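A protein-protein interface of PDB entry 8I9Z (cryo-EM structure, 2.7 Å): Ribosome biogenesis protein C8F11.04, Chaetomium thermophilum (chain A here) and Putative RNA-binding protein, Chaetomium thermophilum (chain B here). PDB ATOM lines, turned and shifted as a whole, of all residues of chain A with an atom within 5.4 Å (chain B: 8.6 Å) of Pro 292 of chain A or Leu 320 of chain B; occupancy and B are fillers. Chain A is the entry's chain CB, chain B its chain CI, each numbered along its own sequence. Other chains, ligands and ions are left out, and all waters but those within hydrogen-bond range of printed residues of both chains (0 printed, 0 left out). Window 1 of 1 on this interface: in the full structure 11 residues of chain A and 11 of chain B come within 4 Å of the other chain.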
ATOM      1  N   PHE A 281      17.644   6.410   4.281  1.00  0.00           N
ATOM      2  CA  PHE A 281      18.019   5.902   2.971  1.00  0.00           C
ATOM      3  C   PHE A 281      17.332   6.716   1.883  1.00  0.00           C
ATOM      4  O   PHE A 281      16.365   7.440   2.130  1.00  0.00           O
ATOM      5  CB  PHE A 281      17.634   4.428   2.809  1.00  0.00           C
ATOM      6  CG  PHE A 281      18.350   3.493   3.738  1.00  0.00           C
ATOM      7  CD1 PHE A 281      19.517   3.868   4.380  1.00  0.00           C
ATOM      8  CD2 PHE A 281      17.852   2.223   3.961  1.00  0.00           C
ATOM      9  CE1 PHE A 281      20.161   3.000   5.230  1.00  0.00           C
ATOM     10  CE2 PHE A 281      18.494   1.352   4.812  1.00  0.00           C
ATOM     11  CZ  PHE A 281      19.653   1.739   5.443  1.00  0.00           C
ATOM     12  N   TYR A 282      17.844   6.582   0.663  1.00  0.00           N
ATOM     13  CA  TYR A 282      17.235   7.224  -0.495  1.00  0.00           C
ATOM     14  C   TYR A 282      17.459   6.328  -1.701  1.00  0.00           C
ATOM     15  O   TYR A 282      18.604   5.987  -2.008  1.00  0.00           O
ATOM     16  CB  TYR A 282      17.834   8.610  -0.752  1.00  0.00           C
ATOM     17  CG  TYR A 282      17.450   9.696   0.225  1.00  0.00           C
ATOM     18  CD1 TYR A 282      18.254   9.989   1.318  1.00  0.00           C
ATOM     19  CD2 TYR A 282      16.302  10.454   0.036  1.00  0.00           C
ATOM     20  CE1 TYR A 282      17.916  10.988   2.207  1.00  0.00           C
ATOM     21  CE2 TYR A 282      15.957  11.457   0.919  1.00  0.00           C
ATOM     22  CZ  TYR A 282      16.768  11.718   2.002  1.00  0.00           C
ATOM     23  OH  TYR A 282      16.428  12.716   2.886  1.00  0.00           O
ATOM     24  N   VAL A 283      16.382   5.942  -2.376  1.00  0.00           N
ATOM     25  CA  VAL A 283      16.503   5.257  -3.658  1.00  0.00           C
ATOM     26  C   VAL A 283      16.736   6.316  -4.725  1.00  0.00           C
ATOM     27  O   VAL A 283      15.912   7.217  -4.911  1.00  0.00           O
ATOM     28  CB  VAL A 283      15.258   4.418  -3.969  1.00  0.00           C
ATOM     29  CG1 VAL A 283      15.595   3.332  -4.973  1.00  0.00           C
ATOM     30  CG2 VAL A 283      14.701   3.811  -2.698  1.00  0.00           C
ATOM     31  N   ALA A 289      15.043  12.590  -8.809  1.00  0.00           N
ATOM     32  CA  ALA A 289      15.167  12.909  -7.396  1.00  0.00           C
ATOM     33  C   ALA A 289      15.195  11.635  -6.552  1.00  0.00           C
ATOM     34  O   ALA A 289      14.987  10.521  -7.041  1.00  0.00           O
ATOM     35  CB  ALA A 289      14.024  13.818  -6.949  1.00  0.00           C
ATOM     36  N   ALA A 290      15.450  11.815  -5.259  1.00  0.00           N
ATOM     37  CA  ALA A 290      15.664  10.711  -4.334  1.00  0.00           C
ATOM     38  C   ALA A 290      14.441  10.522  -3.450  1.00  0.00           C
ATOM     39  O   ALA A 290      13.942  11.485  -2.858  1.00  0.00           O
ATOM     40  CB  ALA A 290      16.905  10.959  -3.475  1.00  0.00           C
ATOM     41  N   LEU A 291      13.966   9.287  -3.362  1.00  0.00           N
ATOM     42  CA  LEU A 291      12.810   8.933  -2.545  1.00  0.00           C
ATOM     43  C   LEU A 291      13.272   8.411  -1.191  1.00  0.00           C
ATOM     44  O   LEU A 291      14.049   7.451  -1.138  1.00  0.00           O
ATOM     45  CB  LEU A 291      11.962   7.878  -3.239  1.00  0.00           C
ATOM     46  CG  LEU A 291      11.529   8.201  -4.671  1.00  0.00           C
ATOM     47  CD1 LEU A 291      10.639   7.103  -5.224  1.00  0.00           C
ATOM     48  CD2 LEU A 291      10.822   9.543  -4.732  1.00  0.00           C
ATOM     49  N   PRO A 292      12.810   8.990  -0.088  1.00  0.00           N
ATOM     50  CA  PRO A 292      13.386   8.664   1.217  1.00  0.00           C
ATOM     51  C   PRO A 292      12.873   7.358   1.799  1.00  0.00           C
ATOM     52  O   PRO A 292      11.731   6.948   1.581  1.00  0.00           O
ATOM     53  CB  PRO A 292      12.958   9.851   2.086  1.00  0.00           C
ATOM     54  CG  PRO A 292      11.655  10.280   1.498  1.00  0.00           C
ATOM     55  CD  PRO A 292      11.680   9.929   0.027  1.00  0.00           C
ATOM     56  N   ILE A 293      13.763   6.695   2.539  1.00  0.00           N
ATOM     57  CA  ILE A 293      13.422   5.585   3.423  1.00  0.00           C
ATOM     58  C   ILE A 293      14.123   5.832   4.755  1.00  0.00           C
ATOM     59  O   ILE A 293      15.317   5.549   4.898  1.00  0.00           O
ATOM     60  CB  ILE A 293      13.833   4.222   2.838  1.00  0.00           C
ATOM     61  CG1 ILE A 293      13.227   3.995   1.455  1.00  0.00           C
ATOM     62  CG2 ILE A 293      13.409   3.098   3.770  1.00  0.00           C
ATOM     63  CD1 ILE A 293      13.787   2.793   0.751  1.00  0.00           C
ATOM     64  N   TYR A 294      13.398   6.362   5.734  1.00  0.00           N
ATOM     65  CA  TYR A 294      14.015   6.774   6.986  1.00  0.00           C
ATOM     66  C   TYR A 294      14.290   5.569   7.881  1.00  0.00           C
ATOM     67  O   TYR A 294      13.600   4.548   7.829  1.00  0.00           O
ATOM     68  CB  TYR A 294      13.117   7.776   7.718  1.00  0.00           C
ATOM     69  CG  TYR A 294      13.794   8.541   8.840  1.00  0.00           C
ATOM     70  CD1 TYR A 294      13.758   8.077  10.149  1.00  0.00           C
ATOM     71  CD2 TYR A 294      14.441   9.743   8.592  1.00  0.00           C
ATOM     72  CE1 TYR A 294      14.366   8.774  11.172  1.00  0.00           C
ATOM     73  CE2 TYR A 294      15.051  10.449   9.611  1.00  0.00           C
ATOM     74  CZ  TYR A 294      15.009   9.959  10.899  1.00  0.00           C
ATOM     75  OH  TYR A 294      15.613  10.658  11.916  1.00  0.00           O
ATOM     76  N   ARG B 313      13.172  18.683   4.970  1.00  0.00           N
ATOM     77  CA  ARG B 313      12.429  17.453   4.728  1.00  0.00           C
ATOM     78  C   ARG B 313      11.046  17.758   4.171  1.00  0.00           C
ATOM     79  O   ARG B 313      10.570  17.066   3.263  1.00  0.00           O
ATOM     80  CB  ARG B 313      12.338  16.635   6.018  1.00  0.00           C
ATOM     81  CG  ARG B 313      11.163  15.677   6.088  1.00  0.00           C
ATOM     82  CD  ARG B 313      10.978  15.125   7.490  1.00  0.00           C
ATOM     83  NE  ARG B 313      12.092  14.273   7.889  1.00  0.00           N
ATOM     84  CZ  ARG B 313      12.932  14.549   8.877  1.00  0.00           C
ATOM     85  NH1 ARG B 313      12.818  15.656   9.592  1.00  0.00           N
ATOM     86  NH2 ARG B 313      13.910  13.692   9.155  1.00  0.00           N
ATOM     87  N   ALA B 314      10.398  18.803   4.691  1.00  0.00           N
ATOM     88  CA  ALA B 314       9.083  19.188   4.190  1.00  0.00           C
ATOM     89  C   ALA B 314       9.161  19.677   2.751  1.00  0.00           C
ATOM     90  O   ALA B 314       8.269  19.395   1.944  1.00  0.00           O
ATOM     91  CB  ALA B 314       8.471  20.262   5.090  1.00  0.00           C
ATOM     92  N   ALA B 315      10.220  20.417   2.415  1.00  0.00           N
ATOM     93  CA  ALA B 315      10.413  20.856   1.038  1.00  0.00           C
ATOM     94  C   ALA B 315      10.659  19.673   0.110  1.00  0.00           C
ATOM     95  O   ALA B 315      10.174  19.657  -1.027  1.00  0.00           O
ATOM     96  CB  ALA B 315      11.572  21.849   0.962  1.00  0.00           C
ATOM     97  N   ARG B 316      11.422  18.679   0.574  1.00  0.00           N
ATOM     98  CA  ARG B 316      11.600  17.459  -0.207  1.00  0.00           C
ATOM     99  C   ARG B 316      10.294  16.687  -0.321  1.00  0.00           C
ATOM    100  O   ARG B 316      10.009  16.088  -1.363  1.00  0.00           O
ATOM    101  CB  ARG B 316      12.683  16.578   0.419  1.00  0.00           C
ATOM    102  CG  ARG B 316      14.102  17.015   0.110  1.00  0.00           C
ATOM    103  CD  ARG B 316      15.106  16.211   0.916  1.00  0.00           C
ATOM    104  NE  ARG B 316      16.346  16.949   1.114  1.00  0.00           N
ATOM    105  CZ  ARG B 316      16.973  17.056   2.278  1.00  0.00           C
ATOM    106  NH1 ARG B 316      16.506  16.479   3.372  1.00  0.00           N
ATOM    107  NH2 ARG B 316      18.099  17.763   2.344  1.00  0.00           N
ATOM    108  N   ALA B 317       9.494  16.682   0.747  1.00  0.00           N
ATOM    109  CA  ALA B 317       8.187  16.038   0.695  1.00  0.00           C
ATOM    110  C   ALA B 317       7.260  16.751  -0.281  1.00  0.00           C
ATOM    111  O   ALA B 317       6.497  16.103  -1.008  1.00  0.00           O
ATOM    112  CB  ALA B 317       7.568  15.995   2.092  1.00  0.00           C
ATOM    113  N   GLU B 318       7.307  18.084  -0.308  1.00  0.00           N
ATOM    114  CA  GLU B 318       6.464  18.835  -1.232  1.00  0.00           C
ATOM    115  C   GLU B 318       6.913  18.629  -2.672  1.00  0.00           C
ATOM    116  O   GLU B 318       6.083  18.529  -3.583  1.00  0.00           O
ATOM    117  CB  GLU B 318       6.471  20.319  -0.869  1.00  0.00           C
ATOM    118  CG  GLU B 318       5.692  20.657   0.395  1.00  0.00           C
ATOM    119  CD  GLU B 318       4.203  20.394   0.257  1.00  0.00           C
ATOM    120  OE1 GLU B 318       3.663  20.576  -0.854  1.00  0.00           O
ATOM    121  OE2 GLU B 318       3.573  20.003   1.262  1.00  0.00           O
ATOM    122  N   LYS B 319       8.225  18.556  -2.897  1.00  0.00           N
ATOM    123  CA  LYS B 319       8.720  18.374  -4.256  1.00  0.00           C
ATOM    124  C   LYS B 319       8.492  16.953  -4.755  1.00  0.00           C
ATOM    125  O   LYS B 319       8.464  16.720  -5.969  1.00  0.00           O
ATOM    126  CB  LYS B 319      10.202  18.754  -4.328  1.00  0.00           C
ATOM    127  CG  LYS B 319      11.181  17.613  -4.091  1.00  0.00           C
ATOM    128  CD  LYS B 319      12.619  18.075  -4.265  1.00  0.00           C
ATOM    129  CE  LYS B 319      13.565  16.897  -4.424  1.00  0.00           C
ATOM    130  NZ  LYS B 319      13.643  16.075  -3.185  1.00  0.00           N
ATOM    131  N   LEU B 320       8.316  15.993  -3.848  1.00  0.00           N
ATOM    132  CA  LEU B 320       8.004  14.629  -4.246  1.00  0.00           C
ATOM    133  C   LEU B 320       6.511  14.345  -4.275  1.00  0.00           C
ATOM    134  O   LEU B 320       6.104  13.293  -4.781  1.00  0.00           O
ATOM    135  CB  LEU B 320       8.695  13.629  -3.315  1.00  0.00           C
ATOM    136  CG  LEU B 320      10.222  13.574  -3.417  1.00  0.00           C
ATOM    137  CD1 LEU B 320      10.782  12.534  -2.465  1.00  0.00           C
ATOM    138  CD2 LEU B 320      10.661  13.296  -4.847  1.00  0.00           C
ATOM    139  N   LYS B 321       5.687  15.245  -3.732  1.00  0.00           N
ATOM    140  CA  LYS B 321       4.245  15.120  -3.910  1.00  0.00           C
ATOM    141  C   LYS B 321       3.859  15.372  -5.360  1.00  0.00           C
ATOM    142  O   LYS B 321       2.957  14.714  -5.894  1.00  0.00           O
ATOM    143  CB  LYS B 321       3.511  16.082  -2.977  1.00  0.00           C
ATOM    144  CG  LYS B 321       3.235  15.515  -1.593  1.00  0.00           C
ATOM    145  CD  LYS B 321       2.395  14.249  -1.668  1.00  0.00           C
ATOM    146  CE  LYS B 321       0.981  14.550  -2.142  1.00  0.00           C
ATOM    147  NZ  LYS B 321       0.151  13.318  -2.234  1.00  0.00           N
ATOM    148  N   GLU B 322       4.532  16.324  -6.012  1.00  0.00           N
ATOM    149  CA  GLU B 322       4.367  16.491  -7.450  1.00  0.00           C
ATOM    150  C   GLU B 322       4.930  15.298  -8.208  1.00  0.00           C
ATOM    151  O   GLU B 322       4.446  14.967  -9.295  1.00  0.00           O
ATOM    152  CB  GLU B 322       5.049  17.780  -7.916  1.00  0.00           C
ATOM    153  CG  GLU B 322       4.252  19.046  -7.646  1.00  0.00           C
ATOM    154  CD  GLU B 322       4.880  19.907  -6.568  1.00  0.00           C
ATOM    155  OE1 GLU B 322       6.060  19.671  -6.231  1.00  0.00           O
ATOM    156  OE2 GLU B 322       4.196  20.819  -6.056  1.00  0.00           O
ATOM    157  N   MET B 323       5.961  14.655  -7.656  1.00  0.00           N
ATOM    158  CA  MET B 323       6.494  13.441  -8.263  1.00  0.00           C
ATOM    159  C   MET B 323       5.485  12.303  -8.193  1.00  0.00           C
ATOM    160  O   MET B 323       5.300  11.564  -9.167  1.00  0.00           O
ATOM    161  CB  MET B 323       7.799  13.049  -7.568  1.00  0.00           C
ATOM    162  CG  MET B 323       8.466  11.810  -8.126  1.00  0.00           C
ATOM    163  SD  MET B 323       8.917  12.008  -9.855  1.00  0.00           S
ATOM    164  CE  MET B 323       9.850  13.539  -9.807  1.00  0.00           C
ATOM    165  N   GLY B 324       4.817  12.151  -7.053  1.00  0.00           N
ATOM    166  CA  GLY B 324       3.842  11.095  -6.889  1.00  0.00           C
ATOM    167  C   GLY B 324       4.179  10.139  -5.766  1.00  0.00           C
ATOM    168  O   GLY B 324       3.776   8.973  -5.797  1.00  0.00           O
ATOM    169  N   TYR B 325       4.921  10.613  -4.768  1.00  0.00           N
ATOM    170  CA  TYR B 325       5.309   9.776  -3.645  1.00  0.00           C
ATOM    171  C   TYR B 325       5.160  10.562  -2.350  1.00  0.00           C
ATOM    172  O   TYR B 325       5.358  11.779  -2.318  1.00  0.00           O
ATOM    173  CB  TYR B 325       6.750   9.274  -3.797  1.00  0.00           C
ATOM    174  CG  TYR B 325       7.205   8.372  -2.676  1.00  0.00           C
ATOM    175  CD1 TYR B 325       6.519   7.202  -2.384  1.00  0.00           C
ATOM    176  CD2 TYR B 325       8.318   8.687  -1.911  1.00  0.00           C
ATOM    177  CE1 TYR B 325       6.924   6.375  -1.361  1.00  0.00           C
ATOM    178  CE2 TYR B 325       8.735   7.863  -0.886  1.00  0.00           C
ATOM    179  CZ  TYR B 325       8.034   6.709  -0.616  1.00  0.00           C
ATOM    180  OH  TYR B 325       8.443   5.883   0.405  1.00  0.00           O
ATOM    181  N   GLU B 326       4.800   9.852  -1.280  1.00  0.00           N
ATOM    182  CA  GLU B 326       4.693  10.442   0.044  1.00  0.00           C
ATOM    183  C   GLU B 326       5.217   9.460   1.084  1.00  0.00           C
ATOM    184  O   GLU B 326       5.136   8.241   0.908  1.00  0.00           O
ATOM    185  CB  GLU B 326       3.247  10.845   0.370  1.00  0.00           C
ATOM    186  CG  GLU B 326       2.254   9.693   0.372  1.00  0.00           C
ATOM    187  CD  GLU B 326       1.580   9.502  -0.973  1.00  0.00           C
ATOM    188  OE1 GLU B 326       2.010  10.143  -1.953  1.00  0.00           O
ATOM    189  OE2 GLU B 326       0.618   8.707  -1.048  1.00  0.00           O
ATOM    190  N   PHE B 327       5.759  10.006   2.169  1.00  0.00           N
ATOM    191  CA  PHE B 327       6.334   9.223   3.255  1.00  0.00           C
ATOM    192  C   PHE B 327       5.608   9.554   4.550  1.00  0.00           C
ATOM    193  O   PHE B 327       5.443  10.730   4.891  1.00  0.00           O
ATOM    194  CB  PHE B 327       7.833   9.502   3.395  1.00  0.00           C
ATOM    195  CG  PHE B 327       8.600   8.386   4.043  1.00  0.00           C
ATOM    196  CD1 PHE B 327       8.884   7.227   3.342  1.00  0.00           C
ATOM    197  CD2 PHE B 327       9.047   8.500   5.349  1.00  0.00           C
ATOM    198  CE1 PHE B 327       9.592   6.197   3.933  1.00  0.00           C
ATOM    199  CE2 PHE B 327       9.757   7.476   5.946  1.00  0.00           C
ATOM    200  CZ  PHE B 327      10.029   6.323   5.236  1.00  0.00           C
ATOM    201  N   GLU B 328       5.177   8.514   5.269  1.00  0.00           N
ATOM    202  CA  GLU B 328       4.389   8.724   6.480  1.00  0.00           C
ATOM    203  C   GLU B 328       5.250   9.245   7.627  1.00  0.00           C
ATOM    204  O   GLU B 328       4.859  10.183   8.332  1.00  0.00           O
ATOM    205  CB  GLU B 328       3.688   7.426   6.881  1.00  0.00           C
ATOM    206  CG  GLU B 328       2.639   6.952   5.888  1.00  0.00           C
ATOM    207  CD  GLU B 328       3.176   5.912   4.925  1.00  0.00           C
ATOM    208  OE1 GLU B 328       4.104   6.233   4.154  1.00  0.00           O
ATOM    209  OE2 GLU B 328       2.666   4.771   4.938  1.00  0.00           O
ATOM    210  N   ALA B 329       6.420   8.651   7.831  1.00  0.00           N
ATOM    211  CA  ALA B 329       7.261   9.001   8.971  1.00  0.00           C
ATOM    212  C   ALA B 329       7.966  10.333   8.758  1.00  0.00           C
ATOM    213  O   ALA B 329       8.454  10.946   9.707  1.00  0.00           O
ATOM    214  CB  ALA B 329       8.275   7.905   9.237  1.00  0.00           C
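Of the printed residues of chain A, Leu 320 of chain B touches Ala 290, Leu 291 and Pro 292. Of the printed residues of chain B, Leu 291 of chain A touches Leu 320 (3.8 Å) and Tyr 325 (3.9 Å). Of the printed residues of chain B, Tyr 282 of chain A touches Arg 316 (3.8 Å). The nearest residue of chain B that does not touch Pro 292 of chain A is Arg 316 of chain B (6.5 Å).
The backbone NH of Tyr 325 of chain B lies within hydrogen-bond range of the backbone carbonyl oxygen of Leu 320 of chain B, 2.9 Å away. The backbone carbonyl oxygen of Ile 293 of chain A sits at hydrogen-bond distance from the backbone NH of Phe 281 of chain A, 2.6 Å away. The backbone carbonyl oxygen of Leu 291 of chain A sits at hydrogen-bond distance from the backbone NH of Val 283 of chain A (3.0 Å).
Along chain A the printed residues that touch a printed residue of chain B span positions 282 to 294. Of the 17 printed residues of chain B, 5 touch a printed residue of chain A.
Arg 316 of chain B touches Tyr 282 of chain A (NH1 to OH, 3.8 Å). Ala 290 of chain A touches Leu 320 of chain B. CD2 of Leu 291 of chain A touches CD1 of Leu 320 of chain B (3.8 Å). Leu 291 of chain A touches Tyr 325 of chain B. Pro 292 of chain A touches Leu 320 of chain B. Pro 292 of chain A touches Tyr 325 of chain B. CE1 of Phe 327 of chain B touches O of Pro 292 of chain A, at 3.3 Å. Ile 293 of chain A touches Phe 327 of chain B (CA to CE1, 3.9 Å). Tyr 294 of chain A touches Arg 313 of chain B. Phe 327 of chain B touches Tyr 294 of chain A.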
